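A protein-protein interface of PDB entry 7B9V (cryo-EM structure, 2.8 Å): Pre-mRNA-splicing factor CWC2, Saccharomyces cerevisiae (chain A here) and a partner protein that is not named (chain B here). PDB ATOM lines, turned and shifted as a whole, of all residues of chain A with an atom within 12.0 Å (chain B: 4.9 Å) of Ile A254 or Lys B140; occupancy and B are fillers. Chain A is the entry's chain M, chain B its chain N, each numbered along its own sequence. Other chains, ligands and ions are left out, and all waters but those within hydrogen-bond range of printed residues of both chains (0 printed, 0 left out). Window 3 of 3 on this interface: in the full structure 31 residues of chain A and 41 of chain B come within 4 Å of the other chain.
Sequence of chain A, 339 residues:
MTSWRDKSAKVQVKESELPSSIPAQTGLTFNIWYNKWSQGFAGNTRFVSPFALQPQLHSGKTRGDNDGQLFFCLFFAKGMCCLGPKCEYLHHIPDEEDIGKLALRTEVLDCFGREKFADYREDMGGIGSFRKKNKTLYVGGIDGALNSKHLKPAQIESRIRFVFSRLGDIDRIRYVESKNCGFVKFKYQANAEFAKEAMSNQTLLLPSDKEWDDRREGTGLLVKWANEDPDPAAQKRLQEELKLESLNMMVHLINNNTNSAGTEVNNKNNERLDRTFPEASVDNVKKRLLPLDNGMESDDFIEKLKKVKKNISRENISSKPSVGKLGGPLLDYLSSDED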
ATOM      1  N   LEU A 244     -12.020   5.641  -6.825  1.00  0.00           N
ATOM      2  CA  LEU A 244     -12.202   4.982  -8.120  1.00  0.00           C
ATOM      3  C   LEU A 244     -13.625   5.166  -8.644  1.00  0.00           C
ATOM      4  O   LEU A 244     -13.824   5.417  -9.841  1.00  0.00           O
ATOM      5  CB  LEU A 244     -11.851   3.498  -8.007  1.00  0.00           C
ATOM      6  CG  LEU A 244     -11.811   2.667  -9.290  1.00  0.00           C
ATOM      7  CD1 LEU A 244     -10.789   3.218 -10.272  1.00  0.00           C
ATOM      8  CD2 LEU A 244     -11.493   1.214  -8.961  1.00  0.00           C
ATOM      9  N   GLU A 245     -14.626   5.011  -7.757  1.00  0.00           N
ATOM     10  CA  GLU A 245     -16.029   5.247  -8.105  1.00  0.00           C
ATOM     11  C   GLU A 245     -16.268   6.691  -8.540  1.00  0.00           C
ATOM     12  O   GLU A 245     -17.001   6.947  -9.512  1.00  0.00           O
ATOM     13  CB  GLU A 245     -16.934   4.883  -6.921  1.00  0.00           C
ATOM     14  CG  GLU A 245     -18.419   5.159  -7.159  1.00  0.00           C
ATOM     15  CD  GLU A 245     -19.311   4.630  -6.055  1.00  0.00           C
ATOM     16  OE1 GLU A 245     -19.016   4.887  -4.870  1.00  0.00           O
ATOM     17  OE2 GLU A 245     -20.317   3.965  -6.383  1.00  0.00           O
ATOM     18  N   SER A 246     -15.622   7.642  -7.846  1.00  0.00           N
ATOM     19  CA  SER A 246     -15.726   9.057  -8.202  1.00  0.00           C
ATOM     20  C   SER A 246     -15.147   9.322  -9.587  1.00  0.00           C
ATOM     21  O   SER A 246     -15.743  10.063 -10.383  1.00  0.00           O
ATOM     22  CB  SER A 246     -15.009   9.901  -7.148  1.00  0.00           C
ATOM     23  OG  SER A 246     -15.234  11.283  -7.335  1.00  0.00           O
ATOM     24  N   LEU A 247     -13.942   8.790  -9.851  1.00  0.00           N
ATOM     25  CA  LEU A 247     -13.294   8.994 -11.147  1.00  0.00           C
ATOM     26  C   LEU A 247     -14.113   8.374 -12.272  1.00  0.00           C
ATOM     27  O   LEU A 247     -14.158   8.917 -13.383  1.00  0.00           O
ATOM     28  CB  LEU A 247     -11.878   8.425 -11.126  1.00  0.00           C
ATOM     29  CG  LEU A 247     -10.866   9.182 -10.266  1.00  0.00           C
ATOM     30  CD1 LEU A 247      -9.662   8.309  -9.954  1.00  0.00           C
ATOM     31  CD2 LEU A 247     -10.438  10.462 -10.962  1.00  0.00           C
ATOM     32  N   ASN A 248     -14.713   7.197 -12.020  1.00  0.00           N
ATOM     33  CA  ASN A 248     -15.572   6.576 -13.025  1.00  0.00           C
ATOM     34  C   ASN A 248     -16.832   7.402 -13.273  1.00  0.00           C
ATOM     35  O   ASN A 248     -17.356   7.407 -14.392  1.00  0.00           O
ATOM     36  CB  ASN A 248     -15.935   5.149 -12.609  1.00  0.00           C
ATOM     37  CG  ASN A 248     -14.740   4.204 -12.656  1.00  0.00           C
ATOM     38  OD1 ASN A 248     -13.759   4.465 -13.349  1.00  0.00           O
ATOM     39  ND2 ASN A 248     -14.825   3.097 -11.923  1.00  0.00           N
ATOM     40  N   MET A 249     -17.317   8.118 -12.245  1.00  0.00           N
ATOM     41  CA  MET A 249     -18.527   8.920 -12.411  1.00  0.00           C
ATOM     42  C   MET A 249     -18.252  10.228 -13.141  1.00  0.00           C
ATOM     43  O   MET A 249     -19.156  10.732 -13.846  1.00  0.00           O
ATOM     44  CB  MET A 249     -19.194   9.148 -11.044  1.00  0.00           C
ATOM     45  CG  MET A 249     -20.500   9.939 -11.084  1.00  0.00           C
ATOM     46  SD  MET A 249     -21.650   9.229 -12.275  1.00  0.00           S
ATOM     47  CE  MET A 249     -21.972   7.626 -11.565  1.00  0.00           C
ATOM     48  N   MET A 250     -17.033  10.785 -12.966  1.00  0.00           N
ATOM     49  CA  MET A 250     -16.640  11.990 -13.702  1.00  0.00           C
ATOM     50  C   MET A 250     -16.780  11.807 -15.205  1.00  0.00           C
ATOM     51  O   MET A 250     -17.219  12.733 -15.887  1.00  0.00           O
ATOM     52  CB  MET A 250     -15.204  12.399 -13.383  1.00  0.00           C
ATOM     53  CG  MET A 250     -14.935  12.819 -11.973  1.00  0.00           C
ATOM     54  SD  MET A 250     -13.296  13.532 -11.798  1.00  0.00           S
ATOM     55  CE  MET A 250     -13.114  13.413 -10.026  1.00  0.00           C
ATOM     56  N   VAL A 251     -16.485  10.591 -15.705  1.00  0.00           N
ATOM     57  CA  VAL A 251     -16.597  10.266 -17.128  1.00  0.00           C
ATOM     58  C   VAL A 251     -18.030  10.468 -17.608  1.00  0.00           C
ATOM     59  O   VAL A 251     -18.274  11.102 -18.642  1.00  0.00           O
ATOM     60  CB  VAL A 251     -16.128   8.820 -17.384  1.00  0.00           C
ATOM     61  CG1 VAL A 251     -16.323   8.430 -18.838  1.00  0.00           C
ATOM     62  CG2 VAL A 251     -14.676   8.626 -16.984  1.00  0.00           C
ATOM     63  N   HIS A 252     -18.998   9.968 -16.820  1.00  0.00           N
ATOM     64  CA  HIS A 252     -20.410  10.086 -17.178  1.00  0.00           C
ATOM     65  C   HIS A 252     -20.875  11.533 -17.162  1.00  0.00           C
ATOM     66  O   HIS A 252     -21.591  11.966 -18.078  1.00  0.00           O
ATOM     67  CB  HIS A 252     -21.272   9.241 -16.236  1.00  0.00           C
ATOM     68  CG  HIS A 252     -21.155   7.769 -16.475  1.00  0.00           C
ATOM     69  ND1 HIS A 252     -20.140   7.004 -15.945  1.00  0.00           N
ATOM     70  CD2 HIS A 252     -21.922   6.924 -17.205  1.00  0.00           C
ATOM     71  CE1 HIS A 252     -20.288   5.749 -16.335  1.00  0.00           C
ATOM     72  NE2 HIS A 252     -21.362   5.676 -17.099  1.00  0.00           N
ATOM     73  N   LEU A 253     -20.521  12.277 -16.089  1.00  0.00           N
ATOM     74  CA  LEU A 253     -20.933  13.682 -16.005  1.00  0.00           C
ATOM     75  C   LEU A 253     -20.348  14.509 -17.146  1.00  0.00           C
ATOM     76  O   LEU A 253     -21.026  15.393 -17.686  1.00  0.00           O
ATOM     77  CB  LEU A 253     -20.579  14.281 -14.639  1.00  0.00           C
ATOM     78  CG  LEU A 253     -21.235  13.702 -13.382  1.00  0.00           C
ATOM     79  CD1 LEU A 253     -20.954  14.596 -12.176  1.00  0.00           C
ATOM     80  CD2 LEU A 253     -22.738  13.549 -13.578  1.00  0.00           C
ATOM     81  N   ILE A 254     -19.076  14.264 -17.494  1.00  0.00           N
ATOM     82  CA  ILE A 254     -18.431  15.036 -18.555  1.00  0.00           C
ATOM     83  C   ILE A 254     -19.045  14.699 -19.908  1.00  0.00           C
ATOM     84  O   ILE A 254     -19.308  15.593 -20.722  1.00  0.00           O
ATOM     85  CB  ILE A 254     -16.907  14.825 -18.513  1.00  0.00           C
ATOM     86  CG1 ILE A 254     -16.349  15.533 -17.292  1.00  0.00           C
ATOM     87  CG2 ILE A 254     -16.184  15.300 -19.777  1.00  0.00           C
ATOM     88  CD1 ILE A 254     -15.087  14.936 -16.872  1.00  0.00           C
ATOM     89  N   ASN A 255     -19.297  13.401 -20.161  1.00  0.00           N
ATOM     90  CA  ASN A 255     -19.810  12.998 -21.466  1.00  0.00           C
ATOM     91  C   ASN A 255     -21.257  13.438 -21.659  1.00  0.00           C
ATOM     92  O   ASN A 255     -21.695  13.642 -22.795  1.00  0.00           O
ATOM     93  CB  ASN A 255     -19.675  11.485 -21.644  1.00  0.00           C
ATOM     94  CG  ASN A 255     -18.226  11.035 -21.747  1.00  0.00           C
ATOM     95  OD1 ASN A 255     -17.332  11.835 -22.019  1.00  0.00           O
ATOM     96  ND2 ASN A 255     -17.989   9.748 -21.518  1.00  0.00           N
ATOM     97  N   ASN A 256     -22.004  13.588 -20.557  1.00  0.00           N
ATOM     98  CA  ASN A 256     -23.375  14.084 -20.610  1.00  0.00           C
ATOM     99  C   ASN A 256     -23.472  15.605 -20.690  1.00  0.00           C
ATOM    100  O   ASN A 256     -24.534  16.120 -21.054  1.00  0.00           O
ATOM    101  CB  ASN A 256     -24.176  13.585 -19.402  1.00  0.00           C
ATOM    102  CG  ASN A 256     -24.401  12.079 -19.428  1.00  0.00           C
ATOM    103  OD1 ASN A 256     -24.145  11.421 -20.430  1.00  0.00           O
ATOM    104  ND2 ASN A 256     -24.855  11.538 -18.309  1.00  0.00           N
ATOM    105  N   ASN A 257     -22.405  16.328 -20.358  1.00  0.00           N
ATOM    106  CA  ASN A 257     -22.444  17.790 -20.322  1.00  0.00           C
ATOM    107  C   ASN A 257     -21.087  18.348 -20.752  1.00  0.00           C
ATOM    108  O   ASN A 257     -20.168  18.470 -19.945  1.00  0.00           O
ATOM    109  CB  ASN A 257     -22.826  18.236 -18.890  1.00  0.00           C
ATOM    110  CG  ASN A 257     -23.124  19.741 -18.754  1.00  0.00           C
ATOM    111  OD1 ASN A 257     -22.990  20.528 -19.686  1.00  0.00           O
ATOM    112  ND2 ASN A 257     -23.569  20.121 -17.560  1.00  0.00           N
ATOM    113  N   VAL B 136     -18.650  20.599 -13.567  1.00  0.00           N
ATOM    114  CA  VAL B 136     -18.270  19.602 -14.588  1.00  0.00           C
ATOM    115  C   VAL B 136     -17.129  20.111 -15.495  1.00  0.00           C
ATOM    116  O   VAL B 136     -16.272  19.307 -15.923  1.00  0.00           O
ATOM    117  CB  VAL B 136     -19.509  19.095 -15.374  1.00  0.00           C
ATOM    118  CG1 VAL B 136     -20.054  20.081 -16.415  1.00  0.00           C
ATOM    119  CG2 VAL B 136     -19.202  17.763 -16.049  1.00  0.00           C
ATOM    120  N   ASP B 137     -17.083  21.428 -15.790  1.00  0.00           N
ATOM    121  CA  ASP B 137     -15.943  21.995 -16.520  1.00  0.00           C
ATOM    122  C   ASP B 137     -14.632  21.801 -15.752  1.00  0.00           C
ATOM    123  O   ASP B 137     -13.591  21.515 -16.355  1.00  0.00           O
ATOM    124  CB  ASP B 137     -16.178  23.482 -16.817  1.00  0.00           C
ATOM    125  CG  ASP B 137     -17.308  23.722 -17.818  1.00  0.00           C
ATOM    126  OD1 ASP B 137     -17.564  22.840 -18.662  1.00  0.00           O
ATOM    127  OD2 ASP B 137     -17.975  24.783 -17.728  1.00  0.00           O
ATOM    128  N   LYS B 138     -14.663  21.966 -14.421  1.00  0.00           N
ATOM    129  CA  LYS B 138     -13.460  21.746 -13.610  1.00  0.00           C
ATOM    130  C   LYS B 138     -13.127  20.247 -13.480  1.00  0.00           C
ATOM    131  O   LYS B 138     -11.939  19.858 -13.382  1.00  0.00           O
ATOM    132  CB  LYS B 138     -13.660  22.424 -12.256  1.00  0.00           C
ATOM    133  CG  LYS B 138     -13.624  23.963 -12.353  1.00  0.00           C
ATOM    134  CD  LYS B 138     -13.846  24.633 -11.007  1.00  0.00           C
ATOM    135  CE  LYS B 138     -12.581  24.631 -10.174  1.00  0.00           C
ATOM    136  NZ  LYS B 138     -12.742  25.392  -8.905  1.00  0.00           N
ATOM    137  N   LEU B 139     -14.166  19.394 -13.427  1.00  0.00           N
ATOM    138  CA  LEU B 139     -13.967  17.943 -13.344  1.00  0.00           C
ATOM    139  C   LEU B 139     -13.237  17.409 -14.573  1.00  0.00           C
ATOM    140  O   LEU B 139     -12.540  16.375 -14.478  1.00  0.00           O
ATOM    141  CB  LEU B 139     -15.312  17.227 -13.147  1.00  0.00           C
ATOM    142  CG  LEU B 139     -16.050  17.293 -11.809  1.00  0.00           C
ATOM    143  CD1 LEU B 139     -17.423  16.673 -11.898  1.00  0.00           C
ATOM    144  CD2 LEU B 139     -15.256  16.475 -10.846  1.00  0.00           C
ATOM    145  N   LYS B 140     -13.458  18.038 -15.750  1.00  0.00           N
ATOM    146  CA  LYS B 140     -12.683  17.639 -16.933  1.00  0.00           C
ATOM    147  C   LYS B 140     -11.185  17.846 -16.726  1.00  0.00           C
ATOM    148  O   LYS B 140     -10.373  17.041 -17.214  1.00  0.00           O
ATOM    149  CB  LYS B 140     -13.165  18.393 -18.175  1.00  0.00           C
ATOM    150  CG  LYS B 140     -12.580  17.848 -19.483  1.00  0.00           C
ATOM    151  CD  LYS B 140     -13.376  18.256 -20.711  1.00  0.00           C
ATOM    152  CE  LYS B 140     -13.257  19.743 -20.969  1.00  0.00           C
ATOM    153  NZ  LYS B 140     -11.856  20.141 -21.280  1.00  0.00           N
ATOM    154  N   ASN B 141     -10.805  18.903 -15.990  1.00  0.00           N
ATOM    155  CA  ASN B 141      -9.401  19.118 -15.666  1.00  0.00           C
ATOM    156  C   ASN B 141      -8.881  18.022 -14.754  1.00  0.00           C
ATOM    157  O   ASN B 141      -7.699  17.661 -14.837  1.00  0.00           O
ATOM    158  CB  ASN B 141      -9.181  20.480 -15.024  1.00  0.00           C
ATOM    159  CG  ASN B 141      -7.717  20.842 -14.940  1.00  0.00           C
ATOM    160  OD1 ASN B 141      -6.932  20.492 -15.820  1.00  0.00           O
ATOM    161  ND2 ASN B 141      -7.332  21.510 -13.861  1.00  0.00           N
ATOM    162  N   ILE B 142      -9.746  17.522 -13.850  1.00  0.00           N
ATOM    163  CA  ILE B 142      -9.311  16.434 -12.958  1.00  0.00           C
ATOM    164  C   ILE B 142      -9.029  15.160 -13.757  1.00  0.00           C
ATOM    165  O   ILE B 142      -8.004  14.493 -13.544  1.00  0.00           O
ATOM    166  CB  ILE B 142     -10.336  16.167 -11.837  1.00  0.00           C
ATOM    167  CG1 ILE B 142     -10.666  17.440 -11.067  1.00  0.00           C
ATOM    168  CG2 ILE B 142      -9.816  15.084 -10.869  1.00  0.00           C
ATOM    169  CD1 ILE B 142      -9.454  18.083 -10.423  1.00  0.00           C
ATOM    170  N   LEU B 143      -9.932  14.808 -14.687  1.00  0.00           N
ATOM    171  CA  LEU B 143      -9.715  13.594 -15.484  1.00  0.00           C
ATOM    172  C   LEU B 143      -8.543  13.744 -16.449  1.00  0.00           C
ATOM    173  O   LEU B 143      -7.887  12.744 -16.778  1.00  0.00           O
ATOM    174  CB  LEU B 143     -10.954  13.155 -16.255  1.00  0.00           C
ATOM    175  CG  LEU B 143     -12.095  12.496 -15.488  1.00  0.00           C
ATOM    176  CD1 LEU B 143     -13.015  11.914 -16.523  1.00  0.00           C
ATOM    177  CD2 LEU B 143     -11.637  11.412 -14.511  1.00  0.00           C
ATOM    178  N   LEU B 144      -8.324  14.964 -16.968  1.00  0.00           N
ATOM    179  CA  LEU B 144      -7.136  15.245 -17.773  1.00  0.00           C
ATOM    180  C   LEU B 144      -5.866  15.037 -16.956  1.00  0.00           C
ATOM    181  O   LEU B 144      -4.892  14.457 -17.449  1.00  0.00           O
ATOM    182  CB  LEU B 144      -7.196  16.668 -18.351  1.00  0.00           C
ATOM    183  CG  LEU B 144      -6.067  17.168 -19.279  1.00  0.00           C
ATOM    184  CD1 LEU B 144      -6.653  18.009 -20.387  1.00  0.00           C
ATOM    185  CD2 LEU B 144      -4.988  18.016 -18.577  1.00  0.00           C
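Of the printed residues of chain B, Leu A247 touches Leu B143. Met A249 touches none of the printed residues of chain B. Printed residues of chain B within 4 Å of Leu A253: Val B136 (3.4 Å). Of the printed residues of chain B, Ile A254 touches Val B136, Leu B139, Lys B140 and Leu B143. Asn A256 touches none of the printed residues of chain B. Of the printed residues of chain B, Asn A257 touches Val B136. Val B136 touches just these residues of chain A: Leu A253, Ile A254 and Asn A257. Lys B140 touches just one residue of chain A: Ile A254. No residue of chain A comes within 4 Å of Asn B141. Ile B142 touches one residue of chain A. Of chain A, only Leu A247 (3.7 Å), Met A250 (3.8 Å), Val A251 (3.7 Å) and Ile A254 (3.7 Å) come within 4 Å of Leu B143. No residue of chain A comes within 4 Å of Leu B144.
Of the 14 printed residues of chain A, 6 touch a printed residue of chain B. Along chain A the printed residues that touch a printed residue of chain B span positions 247 to 257. Of the 9 printed residues of chain B, 5 touch a printed residue of chain A. Hydrophobic or aromatic side chains of chain B that line the printed part of chain A: Val B136, Leu B139, Ile B142 and Leu B143. Among the printed residues, no Asp or Glu carboxylate lies within 4 Å of a Lys or Arg side-chain nitrogen of the other chain.
The backbone carbonyl oxygen of Val A251 lies close to the side-chain amide nitrogen of Asn A255 (3.2 Å).
Among the printed residues, pairs that only touch across the chains: Leu A247 with Leu B143, Met A250 with Leu B139, Met A250 with Ile B142, Met A250 with Leu B143, Val A251 with Leu B143, Leu A253 with Val B136, Ile A254 with Val B136, Ile A254 with Leu B139, Ile A254 with Lys B140, Ile A254 with Leu B143 and Asn A257 with Val B136.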
